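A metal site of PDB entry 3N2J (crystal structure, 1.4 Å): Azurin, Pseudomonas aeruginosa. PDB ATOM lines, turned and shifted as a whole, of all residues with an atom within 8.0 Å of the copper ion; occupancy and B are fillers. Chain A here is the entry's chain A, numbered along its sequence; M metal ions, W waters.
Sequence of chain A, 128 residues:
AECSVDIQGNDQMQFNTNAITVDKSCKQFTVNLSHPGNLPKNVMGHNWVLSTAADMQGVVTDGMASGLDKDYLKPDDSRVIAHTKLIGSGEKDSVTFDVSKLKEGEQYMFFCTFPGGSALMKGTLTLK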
ATOM      1  N   GLN A   8      34.426  10.220  16.790  1.00  0.00           N
ATOM      2  CA  GLN A   8      33.549   9.723  17.827  1.00  0.00           C
ATOM      3  C   GLN A   8      32.854  10.856  18.620  1.00  0.00           C
ATOM      4  O   GLN A   8      33.446  11.912  18.901  1.00  0.00           O
ATOM      5  CB  GLN A   8      34.317   8.836  18.816  1.00  0.00           C
ATOM      6  CG  GLN A   8      34.918   7.564  18.233  1.00  0.00           C
ATOM      7  CD  GLN A   8      35.719   6.736  19.222  1.00  0.00           C
ATOM      8  OE1 GLN A   8      36.072   5.588  18.949  1.00  0.00           O
ATOM      9  NE2 GLN A   8      36.030   7.271  20.399  1.00  0.00           N
ATOM     10  N   GLY A   9      31.610  10.592  19.009  1.00  0.00           N
ATOM     11  CA  GLY A   9      30.875  11.383  19.981  1.00  0.00           C
ATOM     12  C   GLY A   9      30.569  10.479  21.152  1.00  0.00           C
ATOM     13  O   GLY A   9      30.200   9.322  20.944  1.00  0.00           O
ATOM     14  N   ASN A  10      30.677  10.975  22.374  1.00  0.00           N
ATOM     15  CA  ASN A  10      30.422  10.157  23.556  1.00  0.00           C
ATOM     16  C   ASN A  10      29.212  10.609  24.403  1.00  0.00           C
ATOM     17  O   ASN A  10      28.414  11.466  23.995  1.00  0.00           O
ATOM     18  CB  ASN A  10      31.700  10.079  24.396  1.00  0.00           C
ATOM     19  CG  ASN A  10      32.217  11.437  24.825  1.00  0.00           C
ATOM     20  OD1 ASN A  10      31.508  12.473  24.732  1.00  0.00           O
ATOM     21  ND2 ASN A  10      33.472  11.472  25.270  1.00  0.00           N
ATOM     22  N   GLN A  12      29.612  12.234  27.070  1.00  0.00           N
ATOM     23  CA  GLN A  12      30.082  13.510  27.634  1.00  0.00           C
ATOM     24  C   GLN A  12      29.903  14.670  26.605  1.00  0.00           C
ATOM     25  O   GLN A  12      30.432  15.767  26.813  1.00  0.00           O
ATOM     26  CB  GLN A  12      31.564  13.400  28.040  1.00  0.00           C
ATOM     27  CG  GLN A  12      31.804  12.583  29.310  1.00  0.00           C
ATOM     28  CD  GLN A  12      31.405  11.118  29.217  1.00  0.00           C
ATOM     29  OE1 GLN A  12      31.918  10.348  28.388  1.00  0.00           O
ATOM     30  NE2 GLN A  12      30.479  10.707  30.080  1.00  0.00           N
ATOM     31  N   MET A  13      29.199  14.413  25.496  1.00  0.00           N
ATOM     32  CA  MET A  13      28.958  15.405  24.442  1.00  0.00           C
ATOM     33  C   MET A  13      30.245  16.046  23.946  1.00  0.00           C
ATOM     34  O   MET A  13      30.374  17.275  23.870  1.00  0.00           O
ATOM     35  CB  MET A  13      27.875  16.411  24.835  1.00  0.00           C
ATOM     36  CG  MET A  13      26.531  15.768  24.955  1.00  0.00           C
ATOM     37  SD  MET A  13      25.506  16.348  26.308  1.00  0.00           S
ATOM     38  CE  MET A  13      26.388  15.687  27.711  1.00  0.00           C
ATOM     39  N   GLN A  14      31.232  15.192  23.710  1.00  0.00           N
ATOM     40  CA  GLN A  14      32.499  15.611  23.130  1.00  0.00           C
ATOM     41  C   GLN A  14      32.813  14.799  21.873  1.00  0.00           C
ATOM     42  O   GLN A  14      32.545  13.584  21.795  1.00  0.00           O
ATOM     43  CB  GLN A  14      33.639  15.482  24.143  1.00  0.00           C
ATOM     44  CG  GLN A  14      33.475  16.377  25.385  1.00  0.00           C
ATOM     45  CD  GLN A  14      34.328  15.913  26.556  1.00  0.00           C
ATOM     46  OE1 GLN A  14      34.468  14.716  26.829  1.00  0.00           O
ATOM     47  NE2 GLN A  14      34.876  16.863  27.287  1.00  0.00           N
ATOM     48  N   PHE A  15      33.366  15.490  20.874  1.00  0.00           N
ATOM     49  CA  PHE A  15      33.933  14.836  19.719  1.00  0.00           C
ATOM     50  C   PHE A  15      35.386  14.563  20.129  1.00  0.00           C
ATOM     51  O   PHE A  15      35.947  15.316  20.934  1.00  0.00           O
ATOM     52  CB  PHE A  15      33.918  15.742  18.481  1.00  0.00           C
ATOM     53  CG  PHE A  15      32.629  15.869  17.699  1.00  0.00           C
ATOM     54  CD1 PHE A  15      31.967  14.736  17.215  1.00  0.00           C
ATOM     55  CD2 PHE A  15      32.097  17.115  17.411  1.00  0.00           C
ATOM     56  CE1 PHE A  15      30.802  14.859  16.459  1.00  0.00           C
ATOM     57  CE2 PHE A  15      30.924  17.240  16.666  1.00  0.00           C
ATOM     58  CZ  PHE A  15      30.273  16.105  16.203  1.00  0.00           C
ATOM     59  N   LEU A  33      31.541   8.248  11.477  1.00  0.00           N
ATOM     60  CA  LEU A  33      31.120   8.686  12.811  1.00  0.00           C
ATOM     61  C   LEU A  33      30.672   7.503  13.619  1.00  0.00           C
ATOM     62  O   LEU A  33      29.943   6.627  13.106  1.00  0.00           O
ATOM     63  CB  LEU A  33      29.984   9.741  12.726  1.00  0.00           C
ATOM     64  CG  LEU A  33      29.503  10.343  14.073  1.00  0.00           C
ATOM     65  CD1 LEU A  33      30.514  11.358  14.545  1.00  0.00           C
ATOM     66  CD2 LEU A  33      28.109  11.019  13.959  1.00  0.00           C
ATOM     67  N   HIS A  35      29.630   6.075  18.043  1.00  0.00           N
ATOM     68  CA  HIS A  35      29.166   6.520  19.357  1.00  0.00           C
ATOM     69  C   HIS A  35      29.624   5.466  20.377  1.00  0.00           C
ATOM     70  O   HIS A  35      28.921   4.478  20.596  1.00  0.00           O
ATOM     71  CB  HIS A  35      27.635   6.760  19.343  1.00  0.00           C
ATOM     72  CG  HIS A  35      27.073   7.532  20.500  1.00  0.00           C
ATOM     73  ND1 HIS A  35      27.528   7.354  21.800  1.00  0.00           N
ATOM     74  CD2 HIS A  35      26.067   8.437  20.510  1.00  0.00           C
ATOM     75  CE1 HIS A  35      26.800   8.161  22.554  1.00  0.00           C
ATOM     76  NE2 HIS A  35      25.911   8.845  21.819  1.00  0.00           N
ATOM     77  N   MET A  44      21.144  11.223  23.810  1.00  0.00           N
ATOM     78  CA  MET A  44      22.550  11.497  23.535  1.00  0.00           C
ATOM     79  C   MET A  44      22.907  11.289  22.054  1.00  0.00           C
ATOM     80  O   MET A  44      23.982  10.743  21.773  1.00  0.00           O
ATOM     81  CB  MET A  44      23.450  10.625  24.438  1.00  0.00           C
ATOM     82  CG  MET A  44      24.869  11.190  24.666  1.00  0.00           C
ATOM     83  SD  MET A  44      24.972  12.858  25.405  1.00  0.00           S
ATOM     84  CE  MET A  44      24.307  12.570  27.015  1.00  0.00           C
ATOM     85  N   GLY A  45      22.051  11.727  21.134  1.00  0.00           N
ATOM     86  CA  GLY A  45      22.353  11.595  19.715  1.00  0.00           C
ATOM     87  C   GLY A  45      23.466  12.535  19.278  1.00  0.00           C
ATOM     88  O   GLY A  45      23.641  13.602  19.864  1.00  0.00           O
ATOM     89  N   HIS A  46      24.231  12.124  18.284  1.00  0.00           N
ATOM     90  CA  HIS A  46      25.274  12.920  17.666  1.00  0.00           C
ATOM     91  C   HIS A  46      25.133  12.732  16.196  1.00  0.00           C
ATOM     92  O   HIS A  46      24.820  11.634  15.713  1.00  0.00           O
ATOM     93  CB  HIS A  46      26.697  12.465  18.054  1.00  0.00           C
ATOM     94  CG  HIS A  46      26.990  12.497  19.525  1.00  0.00           C
ATOM     95  ND1 HIS A  46      26.804  13.650  20.261  1.00  0.00           N
ATOM     96  CD2 HIS A  46      27.391  11.511  20.356  1.00  0.00           C
ATOM     97  CE1 HIS A  46      27.147  13.350  21.501  1.00  0.00           C
ATOM     98  NE2 HIS A  46      27.514  12.072  21.609  1.00  0.00           N
ATOM     99  N   ASN A  47      25.309  13.815  15.480  1.00  0.00           N
ATOM    100  CA  ASN A  47      25.448  13.761  14.055  1.00  0.00           C
ATOM    101  C   ASN A  47      26.725  14.523  13.710  1.00  0.00           C
ATOM    102  O   ASN A  47      27.355  15.127  14.613  1.00  0.00           O
ATOM    103  CB  ASN A  47      24.211  14.244  13.332  1.00  0.00           C
ATOM    104  CG  ASN A  47      23.769  15.663  13.667  1.00  0.00           C
ATOM    105  OD1 ASN A  47      24.433  16.414  14.383  1.00  0.00           O
ATOM    106  ND2 ASN A  47      22.653  16.074  13.056  1.00  0.00           N
ATOM    107  N   TRP A  48      27.176  14.397  12.470  1.00  0.00           N
ATOM    108  CA  TRP A  48      28.324  15.157  11.953  1.00  0.00           C
ATOM    109  C   TRP A  48      27.797  16.007  10.794  1.00  0.00           C
ATOM    110  O   TRP A  48      27.315  15.451   9.803  1.00  0.00           O
ATOM    111  CB  TRP A  48      29.458  14.236  11.467  1.00  0.00           C
ATOM    112  CG  TRP A  48      30.688  14.989  11.053  1.00  0.00           C
ATOM    113  CD1 TRP A  48      31.759  15.297  11.840  1.00  0.00           C
ATOM    114  CD2 TRP A  48      30.970  15.509   9.757  1.00  0.00           C
ATOM    115  NE1 TRP A  48      32.705  15.965  11.101  1.00  0.00           N
ATOM    116  CE2 TRP A  48      32.259  16.083   9.811  1.00  0.00           C
ATOM    117  CE3 TRP A  48      30.319  15.439   8.509  1.00  0.00           C
ATOM    118  CZ2 TRP A  48      32.840  16.715   8.714  1.00  0.00           C
ATOM    119  CZ3 TRP A  48      30.904  16.043   7.421  1.00  0.00           C
ATOM    120  CH2 TRP A  48      32.162  16.660   7.526  1.00  0.00           C
ATOM    121  N   LEU A  86      21.724  11.047  12.526  1.00  0.00           N
ATOM    122  CA  LEU A  86      21.859  11.126  13.991  1.00  0.00           C
ATOM    123  C   LEU A  86      22.025   9.728  14.582  1.00  0.00           C
ATOM    124  O   LEU A  86      21.216   8.855  14.284  1.00  0.00           O
ATOM    125  CB  LEU A  86      20.606  11.729  14.600  1.00  0.00           C
ATOM    126  CG  LEU A  86      20.721  12.182  16.047  1.00  0.00           C
ATOM    127  CD1 LEU A  86      21.359  13.559  16.082  1.00  0.00           C
ATOM    128  CD2 LEU A  86      19.353  12.217  16.703  1.00  0.00           C
ATOM    129  N   ILE A  87      23.064   9.521  15.404  1.00  0.00           N
ATOM    130  CA  ILE A  87      23.347   8.218  15.968  1.00  0.00           C
ATOM    131  C   ILE A  87      23.301   8.260  17.507  1.00  0.00           C
ATOM    132  O   ILE A  87      23.500   9.317  18.116  1.00  0.00           O
ATOM    133  CB  ILE A  87      24.658   7.584  15.397  1.00  0.00           C
ATOM    134  CG1 ILE A  87      25.919   8.241  15.984  1.00  0.00           C
ATOM    135  CG2 ILE A  87      24.658   7.501  13.853  1.00  0.00           C
ATOM    136  CD1 ILE A  87      27.264   7.677  15.547  1.00  0.00           C
ATOM    137  N   PHE A 111      30.012  20.086  12.957  1.00  0.00           N
ATOM    138  CA  PHE A 111      29.315  20.241  14.211  1.00  0.00           C
ATOM    139  C   PHE A 111      28.168  19.250  14.341  1.00  0.00           C
ATOM    140  O   PHE A 111      27.767  18.630  13.376  1.00  0.00           O
ATOM    141  CB  PHE A 111      28.824  21.704  14.409  1.00  0.00           C
ATOM    142  CG  PHE A 111      28.092  22.234  13.219  1.00  0.00           C
ATOM    143  CD1 PHE A 111      28.782  22.835  12.169  1.00  0.00           C
ATOM    144  CD2 PHE A 111      26.711  22.096  13.111  1.00  0.00           C
ATOM    145  CE1 PHE A 111      28.118  23.262  11.020  1.00  0.00           C
ATOM    146  CE2 PHE A 111      26.047  22.526  11.972  1.00  0.00           C
ATOM    147  CZ  PHE A 111      26.746  23.172  10.959  1.00  0.00           C
ATOM    148  N   CYS A 112      27.628  19.164  15.528  1.00  0.00           N
ATOM    149  CA  CYS A 112      26.507  18.300  15.878  1.00  0.00           C
ATOM    150  C   CYS A 112      25.340  19.230  16.142  1.00  0.00           C
ATOM    151  O   CYS A 112      25.529  20.354  16.634  1.00  0.00           O
ATOM    152  CB  CYS A 112      26.853  17.500  17.115  1.00  0.00           C
ATOM    153  SG  CYS A 112      25.481  16.486  17.813  1.00  0.00           S
ATOM    154  N   THR A 113      24.122  18.780  15.843  1.00  0.00           N
ATOM    155  CA  THR A 113      22.952  19.653  15.999  1.00  0.00           C
ATOM    156  C   THR A 113      22.019  19.152  17.083  1.00  0.00           C
ATOM    157  O   THR A 113      20.991  19.778  17.324  1.00  0.00           O
ATOM    158  CB  THR A 113      22.207  19.862  14.674  1.00  0.00           C
ATOM    159  OG1 THR A 113      21.681  18.609  14.180  1.00  0.00           O
ATOM    160  CG2 THR A 113      23.048  20.545  13.609  1.00  0.00           C
ATOM    161  N   PHE A 114      22.357  18.046  17.736  1.00  0.00           N
ATOM    162  CA  PHE A 114      21.537  17.533  18.828  1.00  0.00           C
ATOM    163  C   PHE A 114      21.491  18.543  19.973  1.00  0.00           C
ATOM    164  O   PHE A 114      22.545  19.013  20.380  1.00  0.00           O
ATOM    165  CB  PHE A 114      22.112  16.210  19.350  1.00  0.00           C
ATOM    166  CG  PHE A 114      21.263  15.621  20.447  1.00  0.00           C
ATOM    167  CD1 PHE A 114      21.498  15.918  21.781  1.00  0.00           C
ATOM    168  CD2 PHE A 114      20.169  14.826  20.139  1.00  0.00           C
ATOM    169  CE1 PHE A 114      20.658  15.430  22.792  1.00  0.00           C
ATOM    170  CE2 PHE A 114      19.329  14.325  21.144  1.00  0.00           C
ATOM    171  CZ  PHE A 114      19.595  14.614  22.468  1.00  0.00           C
ATOM    172  N   PRO A 115      20.307  18.887  20.537  1.00  0.00           N
ATOM    173  CA  PRO A 115      20.283  19.859  21.651  1.00  0.00           C
ATOM    174  C   PRO A 115      20.641  19.199  22.989  1.00  0.00           C
ATOM    175  O   PRO A 115      19.793  18.577  23.654  1.00  0.00           O
ATOM    176  CB  PRO A 115      18.860  20.428  21.617  1.00  0.00           C
ATOM    177  CG  PRO A 115      18.151  19.705  20.483  1.00  0.00           C
ATOM    178  CD  PRO A 115      18.944  18.483  20.157  1.00  0.00           C
ATOM    179  N   GLY A 116      21.919  19.306  23.346  1.00  0.00           N
ATOM    180  CA  GLY A 116      22.480  18.699  24.549  1.00  0.00           C
ATOM    181  C   GLY A 116      22.435  19.545  25.812  1.00  0.00           C
ATOM    182  O   GLY A 116      22.462  19.003  26.918  1.00  0.00           O
ATOM    183  N   LEU A 120      28.076  23.670  22.724  1.00  0.00           N
ATOM    184  CA  LEU A 120      28.049  23.205  21.329  1.00  0.00           C
ATOM    185  C   LEU A 120      29.228  22.307  20.927  1.00  0.00           C
ATOM    186  O   LEU A 120      30.373  22.624  21.243  1.00  0.00           O
ATOM    187  CB  LEU A 120      27.991  24.430  20.378  1.00  0.00           C
ATOM    188  CG  LEU A 120      26.622  24.954  19.912  1.00  0.00           C
ATOM    189  CD1 LEU A 120      25.443  24.166  20.493  1.00  0.00           C
ATOM    190  CD2 LEU A 120      26.474  26.436  20.231  1.00  0.00           C
ATOM    191  N   MET A 121      28.931  21.168  20.245  1.00  0.00           N
ATOM    192  CA  MET A 121      29.895  20.197  19.721  1.00  0.00           C
ATOM    193  C   MET A 121      30.295  20.672  18.328  1.00  0.00           C
ATOM    194  O   MET A 121      29.427  20.761  17.451  1.00  0.00           O
ATOM    195  CB  MET A 121      29.242  18.824  19.643  1.00  0.00           C
ATOM    196  CG  MET A 121      29.121  18.181  20.971  1.00  0.00           C
ATOM    197  SD  MET A 121      28.447  16.526  20.819  1.00  0.00           S
ATOM    198  CE  MET A 121      29.825  15.624  20.175  1.00  0.00           C
ATOM    199  N   LYS A 122      31.554  21.060  18.150  1.00  0.00           N
ATOM    200  CA  LYS A 122      32.015  21.628  16.881  1.00  0.00           C
ATOM    201  C   LYS A 122      33.509  21.462  16.714  1.00  0.00           C
ATOM    202  O   LYS A 122      34.219  21.161  17.671  1.00  0.00           O
ATOM    203  CB  LYS A 122      31.671  23.135  16.781  1.00  0.00           C
ATOM    204  CG  LYS A 122      31.756  23.956  18.097  1.00  0.00           C
ATOM    205  CD  LYS A 122      31.241  25.385  17.906  1.00  0.00           C
ATOM    206  CE  LYS A 122      31.956  26.441  18.718  1.00  0.00           C
ATOM    207  NZ  LYS A 122      31.521  26.426  20.140  1.00  0.00           N
HETATM  208 CU    CU M   1      26.596  15.524  19.451  1.00  0.00          CU
HETATM  209  O   HOH W   1      25.184  18.623  20.139  1.00  0.00           O
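Merely in contact with the copper ion: Gly 45. Of the 25 residues printed, 4 come within 4 Å of the copper ion.
The copper ion is bound by a ring nitrogen (ND1) of His 46 (2.1 Å), the side-chain sulfur of Cys 112 (2.2 Å) and the side-chain sulfur of Met 121 (2.5 Å). The copper ion has three donor atoms within binding distance.
A ring nitrogen (NE2) of His 46 sits at hydrogen-bond distance from the backbone carbonyl oxygen (O) of Asn 10 (2.6 Å). N of Asn 47 lies close to SG of Cys 112, at 3.6 Å. The backbone carbonyl oxygen (O) of His 46 is in hydrogen-bond range of the backbone NH (N) of Ile 87 (2.8 Å). The backbone NH of Phe 114 lies close to the side-chain sulfur of Cys 112 (3.5 Å).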
